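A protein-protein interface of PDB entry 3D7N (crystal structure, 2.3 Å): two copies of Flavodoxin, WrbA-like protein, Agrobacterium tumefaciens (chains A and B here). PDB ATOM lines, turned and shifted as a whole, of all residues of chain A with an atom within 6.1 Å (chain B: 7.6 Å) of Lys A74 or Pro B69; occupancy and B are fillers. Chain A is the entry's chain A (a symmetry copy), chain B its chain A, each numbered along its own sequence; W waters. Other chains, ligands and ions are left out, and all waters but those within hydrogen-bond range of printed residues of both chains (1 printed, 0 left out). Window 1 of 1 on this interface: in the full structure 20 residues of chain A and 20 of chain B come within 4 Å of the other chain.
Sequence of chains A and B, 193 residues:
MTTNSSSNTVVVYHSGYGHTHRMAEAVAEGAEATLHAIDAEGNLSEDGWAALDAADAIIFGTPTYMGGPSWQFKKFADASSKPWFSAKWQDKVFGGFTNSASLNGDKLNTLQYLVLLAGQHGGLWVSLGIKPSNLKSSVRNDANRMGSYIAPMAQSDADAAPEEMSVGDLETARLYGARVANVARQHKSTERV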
ATOM      1  N   PRO A  69      14.862  19.085  -6.517  1.00  0.00           N
ATOM      2  CA  PRO A  69      13.817  18.631  -5.621  1.00  0.00           C
ATOM      3  C   PRO A  69      14.120  19.015  -4.172  1.00  0.00           C
ATOM      4  O   PRO A  69      15.293  19.067  -3.784  1.00  0.00           O
ATOM      5  CB  PRO A  69      13.845  17.119  -5.777  1.00  0.00           C
ATOM      6  CG  PRO A  69      15.171  16.773  -6.208  1.00  0.00           C
ATOM      7  CD  PRO A  69      15.622  17.945  -7.092  1.00  0.00           C
ATOM      8  N   SER A  70      13.088  19.287  -3.386  1.00  0.00           N
ATOM      9  CA  SER A  70      13.295  19.572  -1.973  1.00  0.00           C
ATOM     10  C   SER A  70      14.141  18.498  -1.319  1.00  0.00           C
ATOM     11  O   SER A  70      14.106  17.314  -1.721  1.00  0.00           O
ATOM     12  CB  SER A  70      11.964  19.643  -1.271  1.00  0.00           C
ATOM     13  OG  SER A  70      11.225  18.454  -1.446  1.00  0.00           O
ATOM     14  N   TRP A  71      14.902  18.896  -0.300  1.00  0.00           N
ATOM     15  CA  TRP A  71      15.660  17.933   0.447  1.00  0.00           C
ATOM     16  C   TRP A  71      14.793  16.809   1.009  1.00  0.00           C
ATOM     17  O   TRP A  71      15.237  15.679   1.081  1.00  0.00           O
ATOM     18  CB  TRP A  71      16.482  18.581   1.544  1.00  0.00           C
ATOM     19  CG  TRP A  71      15.750  19.071   2.770  1.00  0.00           C
ATOM     20  CD1 TRP A  71      15.379  20.356   3.039  1.00  0.00           C
ATOM     21  CD2 TRP A  71      15.370  18.293   3.908  1.00  0.00           C
ATOM     22  NE1 TRP A  71      14.784  20.422   4.262  1.00  0.00           N
ATOM     23  CE2 TRP A  71      14.755  19.171   4.820  1.00  0.00           C
ATOM     24  CE3 TRP A  71      15.480  16.927   4.245  1.00  0.00           C
ATOM     25  CZ2 TRP A  71      14.251  18.737   6.064  1.00  0.00           C
ATOM     26  CZ3 TRP A  71      14.963  16.500   5.458  1.00  0.00           C
ATOM     27  CH2 TRP A  71      14.375  17.404   6.363  1.00  0.00           C
ATOM     28  N   GLN A  72      13.563  17.126   1.385  1.00  0.00           N
ATOM     29  CA  GLN A  72      12.647  16.144   1.907  1.00  0.00           C
ATOM     30  C   GLN A  72      12.319  15.105   0.848  1.00  0.00           C
ATOM     31  O   GLN A  72      12.318  13.934   1.133  1.00  0.00           O
ATOM     32  CB  GLN A  72      11.355  16.814   2.407  1.00  0.00           C
ATOM     33  CG  GLN A  72      11.495  17.613   3.707  1.00  0.00           C
ATOM     34  CD  GLN A  72      11.691  19.114   3.460  1.00  0.00           C
ATOM     35  OE1 GLN A  72      12.150  19.543   2.398  1.00  0.00           O
ATOM     36  NE2 GLN A  72      11.377  19.902   4.458  1.00  0.00           N
ATOM     37  N   PHE A  73      12.033  15.526  -0.385  1.00  0.00           N
ATOM     38  CA  PHE A  73      11.878  14.541  -1.473  1.00  0.00           C
ATOM     39  C   PHE A  73      13.119  13.671  -1.702  1.00  0.00           C
ATOM     40  O   PHE A  73      12.991  12.473  -1.847  1.00  0.00           O
ATOM     41  CB  PHE A  73      11.443  15.138  -2.800  1.00  0.00           C
ATOM     42  CG  PHE A  73      11.105  14.083  -3.819  1.00  0.00           C
ATOM     43  CD1 PHE A  73       9.865  13.524  -3.854  1.00  0.00           C
ATOM     44  CD2 PHE A  73      12.063  13.592  -4.660  1.00  0.00           C
ATOM     45  CE1 PHE A  73       9.576  12.553  -4.733  1.00  0.00           C
ATOM     46  CE2 PHE A  73      11.765  12.604  -5.550  1.00  0.00           C
ATOM     47  CZ  PHE A  73      10.529  12.098  -5.583  1.00  0.00           C
ATOM     48  N   LYS A  74      14.308  14.260  -1.712  1.00  0.00           N
ATOM     49  CA  LYS A  74      15.553  13.514  -1.985  1.00  0.00           C
ATOM     50  C   LYS A  74      15.837  12.527  -0.842  1.00  0.00           C
ATOM     51  O   LYS A  74      16.196  11.390  -1.074  1.00  0.00           O
ATOM     52  CB  LYS A  74      16.704  14.498  -2.231  1.00  0.00           C
ATOM     53  CG  LYS A  74      18.008  13.886  -2.649  1.00  0.00           C
ATOM     54  CD  LYS A  74      17.867  13.036  -3.924  1.00  0.00           C
ATOM     55  CE  LYS A  74      19.195  12.608  -4.500  1.00  0.00           C
ATOM     56  NZ  LYS A  74      20.075  11.917  -3.487  1.00  0.00           N
ATOM     57  N   LYS A  75      15.593  12.926   0.402  1.00  0.00           N
ATOM     58  CA  LYS A  75      15.663  11.985   1.544  1.00  0.00           C
ATOM     59  C   LYS A  75      14.761  10.760   1.365  1.00  0.00           C
ATOM     60  O   LYS A  75      15.102   9.642   1.754  1.00  0.00           O
ATOM     61  CB  LYS A  75      15.274  12.683   2.847  1.00  0.00           C
ATOM     62  CG  LYS A  75      15.412  11.778   4.087  1.00  0.00           C
ATOM     63  CD  LYS A  75      15.475  12.595   5.356  1.00  0.00           C
ATOM     64  CE  LYS A  75      15.877  11.771   6.571  1.00  0.00           C
ATOM     65  NZ  LYS A  75      14.710  11.276   7.320  1.00  0.00           N
ATOM     66  N   PHE A  76      13.583  10.976   0.824  1.00  0.00           N
ATOM     67  CA  PHE A  76      12.717   9.865   0.481  1.00  0.00           C
ATOM     68  C   PHE A  76      13.290   9.044  -0.674  1.00  0.00           C
ATOM     69  O   PHE A  76      13.218   7.792  -0.638  1.00  0.00           O
ATOM     70  CB  PHE A  76      11.308  10.345   0.125  1.00  0.00           C
ATOM     71  CG  PHE A  76      10.618   9.462  -0.834  1.00  0.00           C
ATOM     72  CD1 PHE A  76       9.943   8.319  -0.388  1.00  0.00           C
ATOM     73  CD2 PHE A  76      10.635   9.752  -2.200  1.00  0.00           C
ATOM     74  CE1 PHE A  76       9.306   7.458  -1.294  1.00  0.00           C
ATOM     75  CE2 PHE A  76       9.990   8.911  -3.119  1.00  0.00           C
ATOM     76  CZ  PHE A  76       9.349   7.748  -2.673  1.00  0.00           C
ATOM     77  N   ALA A  77      13.836   9.726  -1.696  1.00  0.00           N
ATOM     78  CA  ALA A  77      14.416   9.049  -2.843  1.00  0.00           C
ATOM     79  C   ALA A  77      15.598   8.174  -2.380  1.00  0.00           C
ATOM     80  O   ALA A  77      15.745   6.982  -2.800  1.00  0.00           O
ATOM     81  CB  ALA A  77      14.890  10.086  -3.903  1.00  0.00           C
ATOM     82  N   ASP A  78      16.442   8.772  -1.517  1.00  0.00           N
ATOM     83  CA  ASP A  78      17.592   8.071  -0.982  1.00  0.00           C
ATOM     84  C   ASP A  78      17.111   6.824  -0.219  1.00  0.00           C
ATOM     85  O   ASP A  78      17.707   5.757  -0.341  1.00  0.00           O
ATOM     86  CB  ASP A  78      18.478   8.999  -0.131  1.00  0.00           C
ATOM     87  CG  ASP A  78      19.215  10.040  -0.964  1.00  0.00           C
ATOM     88  OD1 ASP A  78      19.141   9.984  -2.220  1.00  0.00           O
ATOM     89  OD2 ASP A  78      19.908  10.926  -0.387  1.00  0.00           O
ATOM     90  N   ALA A  79      16.015   6.950   0.529  1.00  0.00           N
ATOM     91  CA  ALA A  79      15.467   5.837   1.318  1.00  0.00           C
ATOM     92  C   ALA A  79      14.827   4.772   0.418  1.00  0.00           C
ATOM     93  O   ALA A  79      14.673   3.645   0.821  1.00  0.00           O
ATOM     94  CB  ALA A  79      14.449   6.340   2.351  1.00  0.00           C
ATOM     95  N   TYR A 113      15.461  14.793 -12.676  1.00  0.00           N
ATOM     96  CA  TYR A 113      15.821  13.922 -11.562  1.00  0.00           C
ATOM     97  C   TYR A 113      14.779  12.794 -11.352  1.00  0.00           C
ATOM     98  O   TYR A 113      15.079  11.658 -11.026  1.00  0.00           O
ATOM     99  CB  TYR A 113      16.022  14.680 -10.232  1.00  0.00           C
ATOM    100  CG  TYR A 113      16.269  13.686  -9.106  1.00  0.00           C
ATOM    101  CD1 TYR A 113      15.301  13.385  -8.177  1.00  0.00           C
ATOM    102  CD2 TYR A 113      17.443  12.971  -9.070  1.00  0.00           C
ATOM    103  CE1 TYR A 113      15.541  12.409  -7.152  1.00  0.00           C
ATOM    104  CE2 TYR A 113      17.683  12.001  -8.100  1.00  0.00           C
ATOM    105  CZ  TYR A 113      16.725  11.710  -7.173  1.00  0.00           C
ATOM    106  OH  TYR A 113      17.000  10.740  -6.278  1.00  0.00           O
ATOM    107  N   HIS B  14      29.330  17.103   2.549  1.00  0.00           N
ATOM    108  CA  HIS B  14      28.710  16.006   3.284  1.00  0.00           C
ATOM    109  C   HIS B  14      29.413  14.693   2.906  1.00  0.00           C
ATOM    110  O   HIS B  14      29.725  14.488   1.737  1.00  0.00           O
ATOM    111  CB  HIS B  14      27.183  15.940   3.000  1.00  0.00           C
ATOM    112  CG  HIS B  14      26.535  14.736   3.589  1.00  0.00           C
ATOM    113  ND1 HIS B  14      26.133  13.664   2.824  1.00  0.00           N
ATOM    114  CD2 HIS B  14      26.308  14.384   4.879  1.00  0.00           C
ATOM    115  CE1 HIS B  14      25.650  12.717   3.615  1.00  0.00           C
ATOM    116  NE2 HIS B  14      25.753  13.127   4.867  1.00  0.00           N
ATOM    117  N   GLY B  61      31.065  19.755  -1.656  1.00  0.00           N
ATOM    118  CA  GLY B  61      31.326  18.339  -1.720  1.00  0.00           C
ATOM    119  C   GLY B  61      30.128  17.474  -1.375  1.00  0.00           C
ATOM    120  O   GLY B  61      29.515  17.626  -0.342  1.00  0.00           O
ATOM    121  N   THR B  62      29.809  16.508  -2.219  1.00  0.00           N
ATOM    122  CA  THR B  62      28.729  15.579  -1.844  1.00  0.00           C
ATOM    123  C   THR B  62      28.871  14.251  -2.541  1.00  0.00           C
ATOM    124  O   THR B  62      29.380  14.200  -3.659  1.00  0.00           O
ATOM    125  CB  THR B  62      27.342  16.201  -2.116  1.00  0.00           C
ATOM    126  OG1 THR B  62      26.323  15.225  -1.867  1.00  0.00           O
ATOM    127  CG2 THR B  62      27.222  16.734  -3.583  1.00  0.00           C
ATOM    128  N   PRO B  63      28.447  13.181  -1.879  1.00  0.00           N
ATOM    129  CA  PRO B  63      28.214  11.880  -2.504  1.00  0.00           C
ATOM    130  C   PRO B  63      27.144  11.980  -3.567  1.00  0.00           C
ATOM    131  O   PRO B  63      26.400  12.904  -3.529  1.00  0.00           O
ATOM    132  CB  PRO B  63      27.693  10.991  -1.350  1.00  0.00           C
ATOM    133  CG  PRO B  63      27.861  11.762  -0.091  1.00  0.00           C
ATOM    134  CD  PRO B  63      28.201  13.167  -0.421  1.00  0.00           C
ATOM    135  N   THR B  64      27.107  11.031  -4.497  1.00  0.00           N
ATOM    136  CA  THR B  64      26.044  10.899  -5.461  1.00  0.00           C
ATOM    137  C   THR B  64      25.333   9.687  -4.989  1.00  0.00           C
ATOM    138  O   THR B  64      25.938   8.646  -4.799  1.00  0.00           O
ATOM    139  CB  THR B  64      26.555  10.667  -6.867  1.00  0.00           C
ATOM    140  OG1 THR B  64      27.168  11.867  -7.337  1.00  0.00           O
ATOM    141  CG2 THR B  64      25.390  10.232  -7.874  1.00  0.00           C
ATOM    142  N   TYR B  65      24.063   9.832  -4.737  1.00  0.00           N
ATOM    143  CA  TYR B  65      23.283   8.782  -4.181  1.00  0.00           C
ATOM    144  C   TYR B  65      21.940   8.825  -4.836  1.00  0.00           C
ATOM    145  O   TYR B  65      21.339   9.848  -4.938  1.00  0.00           O
ATOM    146  CB  TYR B  65      23.164   9.004  -2.696  1.00  0.00           C
ATOM    147  CG  TYR B  65      22.718   7.813  -1.937  1.00  0.00           C
ATOM    148  CD1 TYR B  65      23.594   6.813  -1.615  1.00  0.00           C
ATOM    149  CD2 TYR B  65      21.421   7.682  -1.536  1.00  0.00           C
ATOM    150  CE1 TYR B  65      23.181   5.719  -0.914  1.00  0.00           C
ATOM    151  CE2 TYR B  65      21.005   6.608  -0.844  1.00  0.00           C
ATOM    152  CZ  TYR B  65      21.879   5.624  -0.533  1.00  0.00           C
ATOM    153  OH  TYR B  65      21.449   4.543   0.162  1.00  0.00           O
ATOM    154  N   MET B  66      21.490   7.680  -5.286  1.00  0.00           N
ATOM    155  CA  MET B  66      20.296   7.566  -6.067  1.00  0.00           C
ATOM    156  C   MET B  66      20.214   8.657  -7.129  1.00  0.00           C
ATOM    157  O   MET B  66      19.205   9.248  -7.358  1.00  0.00           O
ATOM    158  CB  MET B  66      19.077   7.519  -5.160  1.00  0.00           C
ATOM    159  CG  MET B  66      19.029   6.304  -4.234  1.00  0.00           C
ATOM    160  SD  MET B  66      19.024   4.616  -5.087  1.00  0.00           S
ATOM    161  CE  MET B  66      17.469   4.803  -6.067  1.00  0.00           C
ATOM    162  N   GLY B  67      21.320   8.925  -7.782  1.00  0.00           N
ATOM    163  CA  GLY B  67      21.298   9.780  -8.934  1.00  0.00           C
ATOM    164  C   GLY B  67      21.448  11.262  -8.748  1.00  0.00           C
ATOM    165  O   GLY B  67      21.316  11.980  -9.681  1.00  0.00           O
ATOM    166  N   GLY B  68      21.749  11.701  -7.549  1.00  0.00           N
ATOM    167  CA  GLY B  68      21.829  13.115  -7.234  1.00  0.00           C
ATOM    168  C   GLY B  68      22.594  13.358  -5.950  1.00  0.00           C
ATOM    169  O   GLY B  68      23.083  12.429  -5.372  1.00  0.00           O
ATOM    170  N   PRO B  69      22.741  14.627  -5.528  1.00  0.00           N
ATOM    171  CA  PRO B  69      23.409  14.891  -4.269  1.00  0.00           C
ATOM    172  C   PRO B  69      22.646  14.277  -3.094  1.00  0.00           C
ATOM    173  O   PRO B  69      21.413  14.195  -3.140  1.00  0.00           O
ATOM    174  CB  PRO B  69      23.391  16.407  -4.167  1.00  0.00           C
ATOM    175  CG  PRO B  69      22.278  16.861  -4.955  1.00  0.00           C
ATOM    176  CD  PRO B  69      22.187  15.869  -6.124  1.00  0.00           C
ATOM    177  N   SER B  70      23.361  13.845  -2.064  1.00  0.00           N
ATOM    178  CA  SER B  70      22.697  13.331  -0.875  1.00  0.00           C
ATOM    179  C   SER B  70      21.648  14.303  -0.373  1.00  0.00           C
ATOM    180  O   SER B  70      21.782  15.536  -0.532  1.00  0.00           O
ATOM    181  CB  SER B  70      23.714  13.102   0.213  1.00  0.00           C
ATOM    182  OG  SER B  70      24.434  14.282   0.502  1.00  0.00           O
ATOM    183  N   TRP B  71      20.600  13.761   0.247  1.00  0.00           N
ATOM    184  CA  TRP B  71      19.606  14.606   0.846  1.00  0.00           C
ATOM    185  C   TRP B  71      20.199  15.592   1.849  1.00  0.00           C
ATOM    186  O   TRP B  71      19.724  16.706   1.957  1.00  0.00           O
ATOM    187  CB  TRP B  71      18.482  13.806   1.474  1.00  0.00           C
ATOM    188  CG  TRP B  71      18.772  13.094   2.774  1.00  0.00           C
ATOM    189  CD1 TRP B  71      19.068  11.771   2.931  1.00  0.00           C
ATOM    190  CD2 TRP B  71      18.722  13.657   4.088  1.00  0.00           C
ATOM    191  NE1 TRP B  71      19.217  11.482   4.252  1.00  0.00           N
ATOM    192  CE2 TRP B  71      19.020  12.619   4.991  1.00  0.00           C
ATOM    193  CE3 TRP B  71      18.464  14.949   4.594  1.00  0.00           C
ATOM    194  CZ2 TRP B  71      19.060  12.820   6.387  1.00  0.00           C
ATOM    195  CZ3 TRP B  71      18.528  15.148   5.964  1.00  0.00           C
ATOM    196  CH2 TRP B  71      18.803  14.086   6.847  1.00  0.00           C
ATOM    197  N   GLN B  72      21.239  15.180   2.558  1.00  0.00           N
ATOM    198  CA  GLN B  72      21.896  16.031   3.518  1.00  0.00           C
ATOM    199  C   GLN B  72      22.531  17.225   2.824  1.00  0.00           C
ATOM    200  O   GLN B  72      22.401  18.330   3.286  1.00  0.00           O
ATOM    201  CB  GLN B  72      22.962  15.248   4.303  1.00  0.00           C
ATOM    202  CG  GLN B  72      22.415  14.245   5.325  1.00  0.00           C
ATOM    203  CD  GLN B  72      22.359  12.815   4.775  1.00  0.00           C
ATOM    204  OE1 GLN B  72      22.299  12.585   3.564  1.00  0.00           O
ATOM    205  NE2 GLN B  72      22.342  11.860   5.672  1.00  0.00           N
ATOM    206  N   PHE B  73      23.228  17.010   1.707  1.00  0.00           N
ATOM    207  CA  PHE B  73      23.712  18.160   0.919  1.00  0.00           C
ATOM    208  C   PHE B  73      22.596  19.093   0.436  1.00  0.00           C
ATOM    209  O   PHE B  73      22.730  20.294   0.547  1.00  0.00           O
ATOM    210  CB  PHE B  73      24.587  17.784  -0.264  1.00  0.00           C
ATOM    211  CG  PHE B  73      25.218  18.985  -0.915  1.00  0.00           C
ATOM    212  CD1 PHE B  73      26.379  19.506  -0.434  1.00  0.00           C
ATOM    213  CD2 PHE B  73      24.586  19.641  -1.934  1.00  0.00           C
ATOM    214  CE1 PHE B  73      26.919  20.602  -0.986  1.00  0.00           C
ATOM    215  CE2 PHE B  73      25.137  20.755  -2.491  1.00  0.00           C
ATOM    216  CZ  PHE B  73      26.296  21.223  -2.018  1.00  0.00           C
ATOM    217  N   LYS B  74      21.498  18.550  -0.074  1.00  0.00           N
ATOM    218  CA  LYS B  74      20.397  19.367  -0.622  1.00  0.00           C
ATOM    219  C   LYS B  74      19.715  20.155   0.508  1.00  0.00           C
ATOM    220  O   LYS B  74      19.421  21.324   0.365  1.00  0.00           O
ATOM    221  CB  LYS B  74      19.426  18.474  -1.404  1.00  0.00           C
ATOM    222  CG  LYS B  74      18.322  19.187  -2.128  1.00  0.00           C
ATOM    223  CD  LYS B  74      18.860  20.236  -3.116  1.00  0.00           C
ATOM    224  CE  LYS B  74      17.792  20.794  -4.026  1.00  0.00           C
ATOM    225  NZ  LYS B  74      16.602  21.329  -3.268  1.00  0.00           N
ATOM    226  N   LYS B  75      19.537  19.544   1.675  1.00  0.00           N
ATOM    227  CA  LYS B  75      19.057  20.280   2.868  1.00  0.00           C
ATOM    228  C   LYS B  75      19.930  21.490   3.214  1.00  0.00           C
ATOM    229  O   LYS B  75      19.444  22.536   3.649  1.00  0.00           O
ATOM    230  CB  LYS B  75      19.004  19.359   4.087  1.00  0.00           C
ATOM    231  CG  LYS B  75      18.428  20.045   5.343  1.00  0.00           C
ATOM    232  CD  LYS B  75      17.966  19.028   6.358  1.00  0.00           C
ATOM    233  CE  LYS B  75      17.153  19.646   7.487  1.00  0.00           C
ATOM    234  NZ  LYS B  75      17.983  19.972   8.658  1.00  0.00           N
ATOM    235  N   ALA B  77      21.802  22.999   0.867  1.00  0.00           N
ATOM    236  CA  ALA B  77      21.623  23.878  -0.276  1.00  0.00           C
ATOM    237  C   ALA B  77      20.329  24.697  -0.099  1.00  0.00           C
ATOM    238  O   ALA B  77      20.297  25.946  -0.335  1.00  0.00           O
ATOM    239  CB  ALA B  77      21.566  23.050  -1.593  1.00  0.00           C
ATOM    240  N   THR B  98      32.348  15.264  -6.349  1.00  0.00           N
ATOM    241  CA  THR B  98      31.484  14.179  -5.972  1.00  0.00           C
ATOM    242  C   THR B  98      32.215  12.856  -6.115  1.00  0.00           C
ATOM    243  O   THR B  98      33.249  12.765  -6.727  1.00  0.00           O
ATOM    244  CB  THR B  98      30.113  14.191  -6.762  1.00  0.00           C
ATOM    245  OG1 THR B  98      29.155  13.368  -6.060  1.00  0.00           O
ATOM    246  CG2 THR B  98      30.256  13.703  -8.244  1.00  0.00           C
ATOM    247  N   ASP B 106      25.665   8.978 -13.233  1.00  0.00           N
ATOM    248  CA  ASP B 106      24.966   9.840 -12.336  1.00  0.00           C
ATOM    249  C   ASP B 106      25.768  10.934 -11.718  1.00  0.00           C
ATOM    250  O   ASP B 106      25.215  11.909 -11.295  1.00  0.00           O
ATOM    251  CB  ASP B 106      24.430   8.999 -11.230  1.00  0.00           C
ATOM    252  CG  ASP B 106      23.401   8.061 -11.694  1.00  0.00           C
ATOM    253  OD1 ASP B 106      23.349   6.978 -11.101  1.00  0.00           O
ATOM    254  OD2 ASP B 106      22.643   8.387 -12.628  1.00  0.00           O
ATOM    255  N   ASN B 109      25.216  14.401 -13.076  1.00  0.00           N
ATOM    256  CA  ASN B 109      24.032  15.054 -12.577  1.00  0.00           C
ATOM    257  C   ASN B 109      24.263  15.849 -11.257  1.00  0.00           C
ATOM    258  O   ASN B 109      23.758  16.937 -11.092  1.00  0.00           O
ATOM    259  CB  ASN B 109      22.902  14.047 -12.391  1.00  0.00           C
ATOM    260  CG  ASN B 109      21.564  14.741 -12.121  1.00  0.00           C
ATOM    261  OD1 ASN B 109      21.140  15.561 -12.929  1.00  0.00           O
ATOM    262  ND2 ASN B 109      20.927  14.462 -10.958  1.00  0.00           N
ATOM    263  N   THR B 110      24.978  15.253 -10.334  1.00  0.00           N
ATOM    264  CA  THR B 110      25.353  15.859  -9.063  1.00  0.00           C
ATOM    265  C   THR B 110      26.215  17.087  -9.341  1.00  0.00           C
ATOM    266  O   THR B 110      25.885  18.128  -8.897  1.00  0.00           O
ATOM    267  CB  THR B 110      26.073  14.861  -8.162  1.00  0.00           C
ATOM    268  OG1 THR B 110      25.156  13.808  -7.901  1.00  0.00           O
ATOM    269  CG2 THR B 110      26.506  15.482  -6.808  1.00  0.00           C
ATOM    270  N   LEU B 111      27.183  16.979 -10.235  1.00  0.00           N
ATOM    271  CA  LEU B 111      28.050  18.103 -10.538  1.00  0.00           C
ATOM    272  C   LEU B 111      27.274  19.259 -11.163  1.00  0.00           C
ATOM    273  O   LEU B 111      27.524  20.431 -10.801  1.00  0.00           O
ATOM    274  CB  LEU B 111      29.235  17.676 -11.408  1.00  0.00           C
ATOM    275  CG  LEU B 111      30.209  16.721 -10.697  1.00  0.00           C
ATOM    276  CD1 LEU B 111      31.351  16.290 -11.626  1.00  0.00           C
ATOM    277  CD2 LEU B 111      30.655  17.404  -9.379  1.00  0.00           C
ATOM    278  N   TYR B 113      24.129  19.916 -10.707  1.00  0.00           N
ATOM    279  CA  TYR B 113      23.388  20.596  -9.649  1.00  0.00           C
ATOM    280  C   TYR B 113      24.264  21.640  -8.912  1.00  0.00           C
ATOM    281  O   TYR B 113      23.838  22.713  -8.520  1.00  0.00           O
ATOM    282  CB  TYR B 113      22.773  19.630  -8.614  1.00  0.00           C
ATOM    283  CG  TYR B 113      22.131  20.425  -7.486  1.00  0.00           C
ATOM    284  CD1 TYR B 113      22.719  20.536  -6.248  1.00  0.00           C
ATOM    285  CD2 TYR B 113      20.993  21.159  -7.728  1.00  0.00           C
ATOM    286  CE1 TYR B 113      22.119  21.331  -5.215  1.00  0.00           C
ATOM    287  CE2 TYR B 113      20.412  21.957  -6.747  1.00  0.00           C
ATOM    288  CZ  TYR B 113      20.991  22.058  -5.516  1.00  0.00           C
ATOM    289  OH  TYR B 113      20.401  22.871  -4.615  1.00  0.00           O
ATOM    290  N   LEU B 114      25.494  21.291  -8.696  1.00  0.00           N
ATOM    291  CA  LEU B 114      26.411  22.115  -7.972  1.00  0.00           C
ATOM    292  C   LEU B 114      26.693  23.397  -8.779  1.00  0.00           C
ATOM    293  O   LEU B 114      26.756  24.495  -8.259  1.00  0.00           O
ATOM    294  CB  LEU B 114      27.640  21.243  -7.768  1.00  0.00           C
ATOM    295  CG  LEU B 114      27.816  20.614  -6.382  1.00  0.00           C
ATOM    296  CD1 LEU B 114      26.569  20.339  -5.528  1.00  0.00           C
ATOM    297  CD2 LEU B 114      28.778  19.450  -6.425  1.00  0.00           C
HETATM  298  O   HOH W   1      18.912   5.009   1.930  1.00  0.00           O
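The side-chain amino group (NZ) of Lys B74 sits at hydrogen-bond distance from the backbone carbonyl oxygen (O) of Pro A69 (2.7 Å). The side-chain carboxylate of Asp A78 lies close to the backbone carbonyl oxygen of Tyr B65, 3.5 Å away. O of Tyr B65 is in hydrogen-bond range of NZ of Lys A74 (2.8 Å). The backbone carbonyl oxygen (O) of Pro B69 lies within hydrogen-bond range of the side-chain amino group (NZ) of Lys A74. The backbone NH (N) of Trp B71 lies within hydrogen-bond range of the side-chain carboxylate (OD2) of Asp A78. The side-chain hydroxyl (OH) of Tyr A113 is in hydrogen-bond range of the backbone carbonyl oxygen (O) of Met B66 (2.9 Å).
OG of Ser B70 sits at hydrogen-bond distance from N of Phe B73, at 3.2 Å. O of Gly B67 lies within hydrogen-bond range of ND2 of Asn B109 (2.8 Å). The side-chain hydroxyl (OG) of Ser B70 lies within hydrogen-bond range of the side-chain hydroxyl (OG1) of Thr B62 (3.2 Å). N of Phe A73 lies within hydrogen-bond range of OG of Ser A70 (3.2 Å). The indole nitrogen of Trp A71 sits at hydrogen-bond distance from the side-chain amide oxygen of Gln A72, 3.3 Å away.
Among the printed residues, pairs that only touch across the chains: Ser A70 with Lys B74 (3.96 Å), Trp A71 with Trp B71 (3.6 Å), Trp A71 with Lys B74 (3.7 Å), Trp A71 with Lys B75 (3.2 Å), Lys A74 with Gly B68 (3.6 Å), Lys A74 with Ser B70 (3.96 Å), Lys A74 with Trp B71 (3.7 Å), Lys A75 with Trp B71 (3.2 Å), Ala A77 with Met B66 (3.6 Å), Asp A78 with Met B66 (3.8 Å), Asp A78 with Ser B70 (3.7 Å) and Tyr A113 with Gly B67 (3.9 Å).
Lys A74 touches just these residues of chain B: Tyr B65, Gly B68, Pro B69, Ser B70 and Trp B71. Printed residues of chain B within 4 Å of Lys A75: Trp B71 (3.2 Å). Thr B62 touches none of the printed residues of chain A. Printed residues of chain A within 4 Å of Ser B70: Lys A74 and Asp A78. Printed residues of chain A within 4 Å of Lys B74: Pro A69 (2.7 Å), Ser A70 (3.96 Å) and Trp A71 (3.7 Å). Printed residues of chain A within 4 Å of Lys B75: Trp A71 (3.2 Å). The nearest residue of chain A that does not touch Pro B69 is Asp A78 (4.5 Å).
Of the 12 printed residues of chain A, 8 touch a printed residue of chain B. Printed residues of chain A that touch a printed residue of chain B: Pro A69, Ser A70, Trp A71, Lys A74, Lys A75, Ala A77, Asp A78 and Tyr A113. Along chain A the printed residues that touch a printed residue of chain B span positions 69 to 113. Of the 24 printed residues of chain B, 9 touch a printed residue of chain A. Printed residues of chain B that touch a printed residue of chain A: Tyr B65, Met B66, Gly B67, Gly B68, Pro B69, Ser B70, Trp B71, Lys B74 and Lys B75. Hydrophobic or aromatic side chains of chain B within 4 Å of the printed part of chain A: Tyr B65, Met B66 and Trp B71. Among the printed residues, 18 pairs touch across the chains. Among the printed residues, no Asp or Glu carboxylate lies within 4 Å of a Lys or Arg side-chain nitrogen of the other chain.
Pro A69 touches Lys B74, and with the chains exchanged Lys A74 touches Pro B69. Ser A70 touches Lys B74, and with the chains exchanged Lys A74 touches Ser B70. Trp A71 touches its own counterpart, Trp B71. Trp A71 touches Lys B75, and with the chains exchanged Lys A75 touches Trp B71. 9 positions are printed for both chains.
Water W1 bridges the backbone carbonyl oxygen of Asp A78 (2.7 Å) and the side-chain hydroxyl of Tyr B65 (3.1 Å).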
